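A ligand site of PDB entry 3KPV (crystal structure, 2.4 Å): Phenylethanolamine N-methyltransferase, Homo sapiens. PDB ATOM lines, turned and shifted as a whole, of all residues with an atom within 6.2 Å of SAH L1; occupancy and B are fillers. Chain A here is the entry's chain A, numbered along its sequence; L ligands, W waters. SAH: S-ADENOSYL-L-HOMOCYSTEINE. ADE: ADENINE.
A nitrogen (N) of SAH L1 lies within hydrogen-bond range of the backbone carbonyl oxygen of Gly 79 (2.6 Å).
A nitrogen (N1) of SAH L1 sits at hydrogen-bond distance from the backbone NH (N) of Val 159, 2.7 Å away.
The side-chain carboxylate of Asp 158 sits at hydrogen-bond distance from a nitrogen (N6) of SAH L1 (3.1 Å).
The side-chain carboxylate (OD1) of Asp 101 is in hydrogen-bond range of an oxygen (O3') of SAH L1 (2.6 Å).
A nitrogen (N) of SAH L1 is in hydrogen-bond range of the backbone carbonyl oxygen (O) of Ala 181 (2.8 Å).
O3' of SAH L1 is in hydrogen-bond range of OD1 of Asn 106.
N of SAH L1 lies within hydrogen-bond range of O of Ser 80, 3.1 Å away.
OXT of SAH L1 is in hydrogen-bond range of OH of Tyr 40 (2.6 Å).
N7 of ADE L2 lies close to OH of Tyr 35.
A nitrogen (N3) of SAH L1 is in hydrogen-bond range of the side-chain sulfur of Cys 183, at 3.5 Å.
The side-chain hydroxyl (OH) of Tyr 35 sits at hydrogen-bond distance from an oxygen (OXT) of SAH L1, at 2.6 Å.
OH of Tyr 85 lies within hydrogen-bond range of O of SAH L1 (2.7 Å).
NE2 of His 160 lies close to N6 of SAH L1, 3.4 Å away.
The side-chain amide oxygen (OE1) of Gln 86 sits at hydrogen-bond distance from the side-chain hydroxyl (OG1) of Thr 83 (2.8 Å).
The side-chain hydroxyl of Tyr 27 sits at hydrogen-bond distance from the backbone carbonyl oxygen of Ala 186 (2.5 Å).
The side-chain hydroxyl (OH) of Tyr 40 lies within hydrogen-bond range of the side-chain amino group (NZ) of Lys 57.
The side-chain carboxylate of Asp 101 lies close to the side-chain amide oxygen of Asn 106, 2.8 Å away.
The backbone carbonyl oxygen (O) of Ser 80 is in hydrogen-bond range of the side-chain amide nitrogen (NE2) of Gln 86, at 3.4 Å.
The side-chain hydroxyl (OG1) of Thr 83 is in hydrogen-bond range of the backbone carbonyl oxygen (O) of Ser 80 (3.3 Å).
The side-chain carboxylate (OD1) of Asp 158 is in hydrogen-bond range of the backbone NH (N) of His 160.
The side-chain amide nitrogen (NE2) of Gln 86 lies within hydrogen-bond range of the side-chain carboxylate (OD2) of Asp 77 (2.8 Å).
O of Phe 182 lies close to SD of SAH L1 (3.6 Å).
Tyr 27 touches SAH L1.
CA of Gly 81 touches O3' of SAH L1 (3.0 Å).
Thr 83 touches SAH L1 (OG1 to C, 3.2 Å).
Gln 86 touches SAH L1 (NE2 to N, 3.8 Å).
Phe 102 touches SAH L1.
Leu 103 touches SAH L1 (CD1 to O2', 3.4 Å).
O of Ile 157 touches C2 of SAH L1, 3.7 Å away.
CG1 of Val 187 touches N7 of SAH L1, at 3.4 Å.
Tyr 222 touches SAH L1.
Hydrophobic or aromatic side chains that line SAH L1: Tyr 27, Tyr 35, Tyr 40, Tyr 85, Phe 102, Leu 103, Val 159, His 160, Ala 181, Phe 182 and Val 187.
The nearest printed residue that does not touch SAH L1 is Ala 186 (4.3 Å).
Water W1 lies within hydrogen-bond range of N6 of ADE L2, SD of SAH L1, O of Phe 182 and OH of Tyr 35.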
ATOM      1  N   ALA A  24       2.575   7.571 -21.690  1.00  0.00           N
ATOM      2  CA  ALA A  24       2.904   6.521 -20.738  1.00  0.00           C
ATOM      3  C   ALA A  24       4.232   5.862 -21.124  1.00  0.00           C
ATOM      4  O   ALA A  24       5.259   6.099 -20.493  1.00  0.00           O
ATOM      5  CB  ALA A  24       1.780   5.486 -20.686  1.00  0.00           C
ATOM      6  N   TYR A  27       6.208   8.653 -22.814  1.00  0.00           N
ATOM      7  CA  TYR A  27       7.088   9.487 -21.991  1.00  0.00           C
ATOM      8  C   TYR A  27       8.515   8.956 -21.921  1.00  0.00           C
ATOM      9  O   TYR A  27       9.419   9.655 -21.455  1.00  0.00           O
ATOM     10  CB  TYR A  27       6.501   9.734 -20.598  1.00  0.00           C
ATOM     11  CG  TYR A  27       5.581  10.932 -20.581  1.00  0.00           C
ATOM     12  CD1 TYR A  27       4.204  10.790 -20.610  1.00  0.00           C
ATOM     13  CD2 TYR A  27       6.108  12.226 -20.578  1.00  0.00           C
ATOM     14  CE1 TYR A  27       3.367  11.881 -20.611  1.00  0.00           C
ATOM     15  CE2 TYR A  27       5.278  13.337 -20.587  1.00  0.00           C
ATOM     16  CZ  TYR A  27       3.910  13.163 -20.599  1.00  0.00           C
ATOM     17  OH  TYR A  27       3.074  14.254 -20.614  1.00  0.00           O
ATOM     18  N   PHE A  30      10.475  11.128 -24.253  1.00  0.00           N
ATOM     19  CA  PHE A  30      10.471  12.545 -23.880  1.00  0.00           C
ATOM     20  C   PHE A  30      11.896  13.077 -23.749  1.00  0.00           C
ATOM     21  O   PHE A  30      12.681  12.571 -22.948  1.00  0.00           O
ATOM     22  CB  PHE A  30       9.701  12.681 -22.567  1.00  0.00           C
ATOM     23  CG  PHE A  30       9.650  14.073 -22.020  1.00  0.00           C
ATOM     24  CD1 PHE A  30       8.470  14.796 -22.062  1.00  0.00           C
ATOM     25  CD2 PHE A  30      10.763  14.644 -21.431  1.00  0.00           C
ATOM     26  CE1 PHE A  30       8.411  16.073 -21.542  1.00  0.00           C
ATOM     27  CE2 PHE A  30      10.708  15.918 -20.903  1.00  0.00           C
ATOM     28  CZ  PHE A  30       9.536  16.636 -20.965  1.00  0.00           C
ATOM     29  N   TYR A  35      12.049  19.796 -24.948  1.00  0.00           N
ATOM     30  CA  TYR A  35      10.910  20.356 -24.243  1.00  0.00           C
ATOM     31  C   TYR A  35      11.193  21.772 -23.720  1.00  0.00           C
ATOM     32  O   TYR A  35      10.346  22.656 -23.846  1.00  0.00           O
ATOM     33  CB  TYR A  35      10.494  19.455 -23.092  1.00  0.00           C
ATOM     34  CG  TYR A  35       9.386  20.035 -22.228  1.00  0.00           C
ATOM     35  CD1 TYR A  35       8.060  19.922 -22.600  1.00  0.00           C
ATOM     36  CD2 TYR A  35       9.695  20.689 -21.031  1.00  0.00           C
ATOM     37  CE1 TYR A  35       7.044  20.451 -21.796  1.00  0.00           C
ATOM     38  CE2 TYR A  35       8.691  21.223 -20.234  1.00  0.00           C
ATOM     39  CZ  TYR A  35       7.372  21.093 -20.619  1.00  0.00           C
ATOM     40  OH  TYR A  35       6.375  21.610 -19.821  1.00  0.00           O
ATOM     41  N   ASN A  39       9.391  25.281 -25.236  1.00  0.00           N
ATOM     42  CA  ASN A  39       8.497  25.976 -24.310  1.00  0.00           C
ATOM     43  C   ASN A  39       9.122  27.100 -23.498  1.00  0.00           C
ATOM     44  O   ASN A  39       8.422  28.025 -23.062  1.00  0.00           O
ATOM     45  CB  ASN A  39       7.819  24.964 -23.382  1.00  0.00           C
ATOM     46  CG  ASN A  39       6.843  24.083 -24.115  1.00  0.00           C
ATOM     47  OD1 ASN A  39       5.790  24.528 -24.550  1.00  0.00           O
ATOM     48  ND2 ASN A  39       7.185  22.810 -24.272  1.00  0.00           N
ATOM     49  N   TYR A  40      10.428  27.026 -23.273  1.00  0.00           N
ATOM     50  CA  TYR A  40      11.069  27.988 -22.384  1.00  0.00           C
ATOM     51  C   TYR A  40      12.201  28.753 -23.034  1.00  0.00           C
ATOM     52  O   TYR A  40      12.928  29.493 -22.366  1.00  0.00           O
ATOM     53  CB  TYR A  40      11.492  27.297 -21.090  1.00  0.00           C
ATOM     54  CG  TYR A  40      10.271  26.788 -20.369  1.00  0.00           C
ATOM     55  CD1 TYR A  40       9.866  25.463 -20.480  1.00  0.00           C
ATOM     56  CD2 TYR A  40       9.476  27.654 -19.629  1.00  0.00           C
ATOM     57  CE1 TYR A  40       8.730  25.008 -19.852  1.00  0.00           C
ATOM     58  CE2 TYR A  40       8.340  27.212 -18.994  1.00  0.00           C
ATOM     59  CZ  TYR A  40       7.969  25.887 -19.101  1.00  0.00           C
ATOM     60  OH  TYR A  40       6.821  25.453 -18.468  1.00  0.00           O
ATOM     61  N   LYS A  57       2.199  33.619 -16.495  1.00  0.00           N
ATOM     62  CA  LYS A  57       2.336  32.521 -15.533  1.00  0.00           C
ATOM     63  C   LYS A  57       3.031  32.986 -14.258  1.00  0.00           C
ATOM     64  O   LYS A  57       2.549  32.733 -13.149  1.00  0.00           O
ATOM     65  CB  LYS A  57       3.096  31.355 -16.156  1.00  0.00           C
ATOM     66  CG  LYS A  57       2.381  30.754 -17.359  1.00  0.00           C
ATOM     67  CD  LYS A  57       2.822  29.330 -17.632  1.00  0.00           C
ATOM     68  CE  LYS A  57       4.308  29.253 -17.929  1.00  0.00           C
ATOM     69  NZ  LYS A  57       4.768  27.863 -18.158  1.00  0.00           N
ATOM     70  N   ASP A  77       6.150  20.065  -5.394  1.00  0.00           N
ATOM     71  CA  ASP A  77       5.854  20.365  -6.788  1.00  0.00           C
ATOM     72  C   ASP A  77       5.597  19.051  -7.509  1.00  0.00           C
ATOM     73  O   ASP A  77       6.445  18.172  -7.512  1.00  0.00           O
ATOM     74  CB  ASP A  77       7.020  21.118  -7.427  1.00  0.00           C
ATOM     75  CG  ASP A  77       6.694  21.623  -8.814  1.00  0.00           C
ATOM     76  OD1 ASP A  77       5.513  21.928  -9.081  1.00  0.00           O
ATOM     77  OD2 ASP A  77       7.619  21.710  -9.647  1.00  0.00           O
ATOM     78  N   ILE A  78       4.423  18.941  -8.122  1.00  0.00           N
ATOM     79  CA  ILE A  78       4.028  17.710  -8.803  1.00  0.00           C
ATOM     80  C   ILE A  78       4.316  17.787 -10.290  1.00  0.00           C
ATOM     81  O   ILE A  78       3.804  18.658 -10.979  1.00  0.00           O
ATOM     82  CB  ILE A  78       2.515  17.433  -8.643  1.00  0.00           C
ATOM     83  CG1 ILE A  78       2.056  17.600  -7.192  1.00  0.00           C
ATOM     84  CG2 ILE A  78       2.156  16.061  -9.210  1.00  0.00           C
ATOM     85  CD1 ILE A  78       2.731  16.661  -6.215  1.00  0.00           C
ATOM     86  N   GLY A  79       5.127  16.861 -10.785  1.00  0.00           N
ATOM     87  CA  GLY A  79       5.454  16.833 -12.195  1.00  0.00           C
ATOM     88  C   GLY A  79       6.305  18.016 -12.590  1.00  0.00           C
ATOM     89  O   GLY A  79       6.001  18.730 -13.561  1.00  0.00           O
ATOM     90  N   SER A  80       7.390  18.219 -11.846  1.00  0.00           N
ATOM     91  CA  SER A  80       8.304  19.324 -12.063  1.00  0.00           C
ATOM     92  C   SER A  80       8.853  19.374 -13.488  1.00  0.00           C
ATOM     93  O   SER A  80       9.064  20.464 -14.045  1.00  0.00           O
ATOM     94  CB  SER A  80       9.476  19.246 -11.077  1.00  0.00           C
ATOM     95  OG  SER A  80       9.012  19.178  -9.743  1.00  0.00           O
ATOM     96  N   GLY A  81       9.076  18.205 -14.073  1.00  0.00           N
ATOM     97  CA  GLY A  81       9.766  18.123 -15.345  1.00  0.00           C
ATOM     98  C   GLY A  81      11.173  18.665 -15.145  1.00  0.00           C
ATOM     99  O   GLY A  81      11.745  18.541 -14.075  1.00  0.00           O
ATOM    100  N   PRO A  82      11.735  19.275 -16.190  1.00  0.00           N
ATOM    101  CA  PRO A  82      13.061  19.864 -16.055  1.00  0.00           C
ATOM    102  C   PRO A  82      12.980  21.365 -15.784  1.00  0.00           C
ATOM    103  O   PRO A  82      13.876  22.089 -16.222  1.00  0.00           O
ATOM    104  CB  PRO A  82      13.659  19.645 -17.441  1.00  0.00           C
ATOM    105  CG  PRO A  82      12.458  19.777 -18.367  1.00  0.00           C
ATOM    106  CD  PRO A  82      11.224  19.396 -17.573  1.00  0.00           C
ATOM    107  N   THR A  83      11.932  21.826 -15.110  1.00  0.00           N
ATOM    108  CA  THR A  83      11.760  23.272 -14.925  1.00  0.00           C
ATOM    109  C   THR A  83      11.658  23.676 -13.444  1.00  0.00           C
ATOM    110  O   THR A  83      11.182  22.894 -12.622  1.00  0.00           O
ATOM    111  CB  THR A  83      10.555  23.843 -15.755  1.00  0.00           C
ATOM    112  OG1 THR A  83       9.305  23.564 -15.092  1.00  0.00           O
ATOM    113  CG2 THR A  83      10.528  23.244 -17.159  1.00  0.00           C
ATOM    114  N   TYR A  85      10.903  27.355 -12.727  1.00  0.00           N
ATOM    115  CA  TYR A  85      10.266  28.684 -12.699  1.00  0.00           C
ATOM    116  C   TYR A  85       9.045  28.692 -11.805  1.00  0.00           C
ATOM    117  O   TYR A  85       8.722  29.711 -11.192  1.00  0.00           O
ATOM    118  CB  TYR A  85       9.838  29.115 -14.109  1.00  0.00           C
ATOM    119  CG  TYR A  85       8.640  28.342 -14.589  1.00  0.00           C
ATOM    120  CD1 TYR A  85       7.354  28.836 -14.444  1.00  0.00           C
ATOM    121  CD2 TYR A  85       8.798  27.083 -15.164  1.00  0.00           C
ATOM    122  CE1 TYR A  85       6.238  28.113 -14.874  1.00  0.00           C
ATOM    123  CE2 TYR A  85       7.705  26.356 -15.598  1.00  0.00           C
ATOM    124  CZ  TYR A  85       6.424  26.871 -15.447  1.00  0.00           C
ATOM    125  OH  TYR A  85       5.354  26.128 -15.879  1.00  0.00           O
ATOM    126  N   GLN A  86       8.352  27.551 -11.764  1.00  0.00           N
ATOM    127  CA  GLN A  86       7.105  27.438 -11.019  1.00  0.00           C
ATOM    128  C   GLN A  86       7.290  27.540  -9.503  1.00  0.00           C
ATOM    129  O   GLN A  86       6.322  27.476  -8.760  1.00  0.00           O
ATOM    130  CB  GLN A  86       6.334  26.164 -11.410  1.00  0.00           C
ATOM    131  CG  GLN A  86       6.991  24.825 -11.001  1.00  0.00           C
ATOM    132  CD  GLN A  86       7.988  24.307 -12.034  1.00  0.00           C
ATOM    133  OE1 GLN A  86       8.499  25.064 -12.853  1.00  0.00           O
ATOM    134  NE2 GLN A  86       8.258  23.013 -11.986  1.00  0.00           N
ATOM    135  N   ASP A 101       9.313  14.235 -10.378  1.00  0.00           N
ATOM    136  CA  ASP A 101       8.923  13.879 -11.746  1.00  0.00           C
ATOM    137  C   ASP A 101       8.957  12.372 -11.951  1.00  0.00           C
ATOM    138  O   ASP A 101       9.583  11.649 -11.183  1.00  0.00           O
ATOM    139  CB  ASP A 101       9.793  14.578 -12.790  1.00  0.00           C
ATOM    140  CG  ASP A 101       9.147  14.573 -14.163  1.00  0.00           C
ATOM    141  OD1 ASP A 101       8.100  15.244 -14.318  1.00  0.00           O
ATOM    142  OD2 ASP A 101       9.668  13.895 -15.070  1.00  0.00           O
ATOM    143  N   PHE A 102       8.279  11.921 -12.997  1.00  0.00           N
ATOM    144  CA  PHE A 102       8.167  10.509 -13.318  1.00  0.00           C
ATOM    145  C   PHE A 102       9.423  10.002 -14.034  1.00  0.00           C
ATOM    146  O   PHE A 102       9.765   8.815 -13.952  1.00  0.00           O
ATOM    147  CB  PHE A 102       6.913  10.283 -14.171  1.00  0.00           C
ATOM    148  CG  PHE A 102       6.731   8.868 -14.656  1.00  0.00           C
ATOM    149  CD1 PHE A 102       6.158   7.911 -13.846  1.00  0.00           C
ATOM    150  CD2 PHE A 102       7.109   8.517 -15.939  1.00  0.00           C
ATOM    151  CE1 PHE A 102       5.985   6.610 -14.304  1.00  0.00           C
ATOM    152  CE2 PHE A 102       6.937   7.229 -16.404  1.00  0.00           C
ATOM    153  CZ  PHE A 102       6.375   6.275 -15.587  1.00  0.00           C
ATOM    154  N   LEU A 103      10.111  10.909 -14.710  1.00  0.00           N
ATOM    155  CA  LEU A 103      11.297  10.552 -15.486  1.00  0.00           C
ATOM    156  C   LEU A 103      12.612  10.864 -14.772  1.00  0.00           C
ATOM    157  O   LEU A 103      12.805  11.950 -14.215  1.00  0.00           O
ATOM    158  CB  LEU A 103      11.287  11.249 -16.839  1.00  0.00           C
ATOM    159  CG  LEU A 103      10.233  10.767 -17.837  1.00  0.00           C
ATOM    160  CD1 LEU A 103      10.123  11.721 -19.006  1.00  0.00           C
ATOM    161  CD2 LEU A 103      10.564   9.356 -18.291  1.00  0.00           C
ATOM    162  N   ASN A 106      14.433  13.943 -16.356  1.00  0.00           N
ATOM    163  CA  ASN A 106      13.984  15.237 -15.832  1.00  0.00           C
ATOM    164  C   ASN A 106      14.615  15.524 -14.489  1.00  0.00           C
ATOM    165  O   ASN A 106      15.076  16.631 -14.240  1.00  0.00           O
ATOM    166  CB  ASN A 106      12.458  15.291 -15.716  1.00  0.00           C
ATOM    167  CG  ASN A 106      11.788  15.606 -17.027  1.00  0.00           C
ATOM    168  OD1 ASN A 106      10.620  15.300 -17.237  1.00  0.00           O
ATOM    169  ND2 ASN A 106      12.540  16.222 -17.932  1.00  0.00           N
ATOM    170  N   ILE A 157       7.725   9.969  -8.901  1.00  0.00           N
ATOM    171  CA  ILE A 157       6.307  10.148  -8.649  1.00  0.00           C
ATOM    172  C   ILE A 157       5.516   9.637  -9.833  1.00  0.00           C
ATOM    173  O   ILE A 157       5.950   9.754 -10.979  1.00  0.00           O
ATOM    174  CB  ILE A 157       5.967  11.636  -8.396  1.00  0.00           C
ATOM    175  CG1 ILE A 157       4.480  11.800  -8.094  1.00  0.00           C
ATOM    176  CG2 ILE A 157       6.375  12.484  -9.582  1.00  0.00           C
ATOM    177  CD1 ILE A 157       4.074  13.235  -7.825  1.00  0.00           C
ATOM    178  N   ASP A 158       4.352   9.060  -9.560  1.00  0.00           N
ATOM    179  CA  ASP A 158       3.453   8.605 -10.607  1.00  0.00           C
ATOM    180  C   ASP A 158       2.040   8.919 -10.173  1.00  0.00           C
ATOM    181  O   ASP A 158       1.468   8.227  -9.319  1.00  0.00           O
ATOM    182  CB  ASP A 158       3.600   7.093 -10.836  1.00  0.00           C
ATOM    183  CG  ASP A 158       2.663   6.569 -11.906  1.00  0.00           C
ATOM    184  OD1 ASP A 158       1.728   7.308 -12.308  1.00  0.00           O
ATOM    185  OD2 ASP A 158       2.861   5.423 -12.359  1.00  0.00           O
ATOM    186  N   VAL A 159       1.477   9.968 -10.764  1.00  0.00           N
ATOM    187  CA  VAL A 159       0.165  10.444 -10.352  1.00  0.00           C
ATOM    188  C   VAL A 159      -0.898   9.379 -10.562  1.00  0.00           C
ATOM    189  O   VAL A 159      -1.959   9.422  -9.938  1.00  0.00           O
ATOM    190  CB  VAL A 159      -0.210  11.735 -11.086  1.00  0.00           C
ATOM    191  CG1 VAL A 159       0.761  12.844 -10.714  1.00  0.00           C
ATOM    192  CG2 VAL A 159      -0.216  11.506 -12.588  1.00  0.00           C
ATOM    193  N   HIS A 160      -0.624   8.420 -11.438  1.00  0.00           N
ATOM    194  CA  HIS A 160      -1.571   7.362 -11.694  1.00  0.00           C
ATOM    195  C   HIS A 160      -1.669   6.383 -10.531  1.00  0.00           C
ATOM    196  O   HIS A 160      -2.559   5.527 -10.502  1.00  0.00           O
ATOM    197  CB  HIS A 160      -1.231   6.634 -13.002  1.00  0.00           C
ATOM    198  CG  HIS A 160      -1.205   7.531 -14.199  1.00  0.00           C
ATOM    199  ND1 HIS A 160      -2.148   8.511 -14.408  1.00  0.00           N
ATOM    200  CD2 HIS A 160      -0.356   7.597 -15.253  1.00  0.00           C
ATOM    201  CE1 HIS A 160      -1.873   9.144 -15.538  1.00  0.00           C
ATOM    202  NE2 HIS A 160      -0.798   8.608 -16.073  1.00  0.00           N
ATOM    203  N   SER A 180       1.627  22.383  -9.218  1.00  0.00           N
ATOM    204  CA  SER A 180       1.738  21.504 -10.374  1.00  0.00           C
ATOM    205  C   SER A 180       1.419  22.231 -11.652  1.00  0.00           C
ATOM    206  O   SER A 180       0.353  22.830 -11.793  1.00  0.00           O
ATOM    207  CB  SER A 180       0.823  20.282 -10.254  1.00  0.00           C
ATOM    208  OG  SER A 180       0.836  19.549 -11.480  1.00  0.00           O
ATOM    209  N   ALA A 181       2.339  22.144 -12.610  1.00  0.00           N
ATOM    210  CA  ALA A 181       2.185  22.852 -13.863  1.00  0.00           C
ATOM    211  C   ALA A 181       2.357  21.919 -15.048  1.00  0.00           C
ATOM    212  O   ALA A 181       3.421  21.338 -15.234  1.00  0.00           O
ATOM    213  CB  ALA A 181       3.178  24.029 -13.939  1.00  0.00           C
ATOM    214  N   PHE A 182       1.286  21.793 -15.828  1.00  0.00           N
ATOM    215  CA  PHE A 182       1.314  21.051 -17.081  1.00  0.00           C
ATOM    216  C   PHE A 182       1.620  19.577 -16.876  1.00  0.00           C
ATOM    217  O   PHE A 182       2.279  18.957 -17.713  1.00  0.00           O
ATOM    218  CB  PHE A 182       2.313  21.681 -18.076  1.00  0.00           C
ATOM    219  CG  PHE A 182       2.034  23.128 -18.377  1.00  0.00           C
ATOM    220  CD1 PHE A 182       2.752  24.134 -17.737  1.00  0.00           C
ATOM    221  CD2 PHE A 182       1.052  23.485 -19.294  1.00  0.00           C
ATOM    222  CE1 PHE A 182       2.488  25.472 -18.014  1.00  0.00           C
ATOM    223  CE2 PHE A 182       0.788  24.810 -19.577  1.00  0.00           C
ATOM    224  CZ  PHE A 182       1.511  25.812 -18.929  1.00  0.00           C
ATOM    225  N   CYS A 183       1.139  19.030 -15.775  1.00  0.00           N
ATOM    226  CA  CYS A 183       1.313  17.597 -15.527  1.00  0.00           C
ATOM    227  C   CYS A 183       0.029  16.789 -15.787  1.00  0.00           C
ATOM    228  O   CYS A 183      -0.063  16.057 -16.775  1.00  0.00           O
ATOM    229  CB  CYS A 183       1.816  17.346 -14.113  1.00  0.00           C
ATOM    230  SG  CYS A 183       2.174  15.619 -13.733  1.00  0.00           S
ATOM    231  N   LEU A 184      -0.948  16.919 -14.899  1.00  0.00           N
ATOM    232  CA  LEU A 184      -2.139  16.071 -14.929  1.00  0.00           C
ATOM    233  C   LEU A 184      -2.717  15.873 -16.340  1.00  0.00           C
ATOM    234  O   LEU A 184      -2.757  14.763 -16.853  1.00  0.00           O
ATOM    235  CB  LEU A 184      -3.220  16.603 -13.990  1.00  0.00           C
ATOM    236  CG  LEU A 184      -2.825  16.916 -12.557  1.00  0.00           C
ATOM    237  CD1 LEU A 184      -4.068  17.115 -11.733  1.00  0.00           C
ATOM    238  CD2 LEU A 184      -1.970  15.796 -11.984  1.00  0.00           C
ATOM    239  N   ALA A 186      -1.523  16.535 -19.057  1.00  0.00           N
ATOM    240  CA  ALA A 186      -0.480  16.089 -19.966  1.00  0.00           C
ATOM    241  C   ALA A 186      -0.156  14.593 -19.823  1.00  0.00           C
ATOM    242  O   ALA A 186       0.554  14.035 -20.649  1.00  0.00           O
ATOM    243  CB  ALA A 186       0.785  16.925 -19.744  1.00  0.00           C
ATOM    244  N   VAL A 187      -0.673  13.964 -18.766  1.00  0.00           N
ATOM    245  CA  VAL A 187      -0.408  12.552 -18.502  1.00  0.00           C
ATOM    246  C   VAL A 187      -1.687  11.713 -18.469  1.00  0.00           C
ATOM    247  O   VAL A 187      -1.673  10.546 -18.073  1.00  0.00           O
ATOM    248  CB  VAL A 187       0.363  12.348 -17.162  1.00  0.00           C
ATOM    249  CG1 VAL A 187       1.609  13.230 -17.099  1.00  0.00           C
ATOM    250  CG2 VAL A 187      -0.546  12.612 -15.965  1.00  0.00           C
ATOM    251  N   TYR A 222       1.358  17.420 -27.673  1.00  0.00           N
ATOM    252  CA  TYR A 222       2.522  18.304 -27.711  1.00  0.00           C
ATOM    253  C   TYR A 222       3.767  17.464 -27.966  1.00  0.00           C
ATOM    254  O   TYR A 222       3.745  16.257 -27.735  1.00  0.00           O
ATOM    255  CB  TYR A 222       2.649  19.169 -26.445  1.00  0.00           C
ATOM    256  CG  TYR A 222       3.154  18.448 -25.220  1.00  0.00           C
ATOM    257  CD1 TYR A 222       4.492  18.553 -24.847  1.00  0.00           C
ATOM    258  CD2 TYR A 222       2.309  17.683 -24.421  1.00  0.00           C
ATOM    259  CE1 TYR A 222       4.983  17.908 -23.717  1.00  0.00           C
ATOM    260  CE2 TYR A 222       2.794  17.029 -23.291  1.00  0.00           C
ATOM    261  CZ  TYR A 222       4.129  17.150 -22.947  1.00  0.00           C
ATOM    262  OH  TYR A 222       4.633  16.520 -21.830  1.00  0.00           O
HETATM  263  N   SAH L   1       6.121  21.200 -14.499  1.00  0.00           N
HETATM  264  CA  SAH L   1       6.663  21.276 -15.854  1.00  0.00           C
HETATM  265  CB  SAH L   1       5.799  20.347 -16.723  1.00  0.00           C
HETATM  266  CG  SAH L   1       6.666  19.239 -17.308  1.00  0.00           C
HETATM  267  SD  SAH L   1       5.734  18.455 -18.657  1.00  0.00           S
HETATM  268  C   SAH L   1       6.491  22.719 -16.358  1.00  0.00           C
HETATM  269  O   SAH L   1       5.791  23.464 -15.755  1.00  0.00           O
HETATM  270  OXT SAH L   1       6.803  23.016 -17.683  1.00  0.00           O
HETATM  271  C5' SAH L   1       4.747  17.086 -17.993  1.00  0.00           C
HETATM  272  C4' SAH L   1       5.557  16.329 -16.921  1.00  0.00           C
HETATM  273  O4' SAH L   1       4.790  15.215 -16.377  1.00  0.00           O
HETATM  274  C3' SAH L   1       6.829  15.719 -17.505  1.00  0.00           C
HETATM  275  O3' SAH L   1       7.954  16.138 -16.755  1.00  0.00           O
HETATM  276  C2' SAH L   1       6.607  14.240 -17.360  1.00  0.00           C
HETATM  277  O2' SAH L   1       7.814  13.531 -17.238  1.00  0.00           O
HETATM  278  C1' SAH L   1       5.777  14.175 -16.084  1.00  0.00           C
HETATM  279  N9  SAH L   1       5.069  12.910 -16.070  1.00  0.00           N
HETATM  280  C8  SAH L   1       4.862  12.011 -17.237  1.00  0.00           C
HETATM  281  N7  SAH L   1       4.053  10.882 -16.788  1.00  0.00           N
HETATM  282  C5  SAH L   1       3.753  11.073 -15.365  1.00  0.00           C
HETATM  283  C6  SAH L   1       2.971  10.242 -14.381  1.00  0.00           C
HETATM  284  N6  SAH L   1       2.331   9.000 -14.815  1.00  0.00           N
HETATM  285  N1  SAH L   1       2.832  10.689 -12.997  1.00  0.00           N
HETATM  286  C2  SAH L   1       3.476  11.976 -12.556  1.00  0.00           C
HETATM  287  N3  SAH L   1       4.257  12.783 -13.526  1.00  0.00           N
HETATM  288  C4  SAH L   1       4.392  12.340 -14.917  1.00  0.00           C
HETATM  289  N9  ADE L   2       4.123  24.766 -21.417  1.00  0.00           N
HETATM  290  C8  ADE L   2       4.616  23.712 -20.704  1.00  0.00           C
HETATM  291  N7  ADE L   2       4.000  22.563 -21.146  1.00  0.00           N
HETATM  292  C5  ADE L   2       3.152  22.914 -22.127  1.00  0.00           C
HETATM  293  C6  ADE L   2       2.275  22.150 -22.916  1.00  0.00           C
HETATM  294  N6  ADE L   2       2.158  20.705 -22.718  1.00  0.00           N
HETATM  295  N1  ADE L   2       1.514  22.768 -23.845  1.00  0.00           N
HETATM  296  C2  ADE L   2       1.599  24.136 -24.009  1.00  0.00           C
HETATM  297  N3  ADE L   2       2.448  24.896 -23.229  1.00  0.00           N
HETATM  298  C4  ADE L   2       3.226  24.278 -22.299  1.00  0.00           C
HETATM  299  O   HOH W   1       3.584  19.709 -20.613  1.00  0.00           O
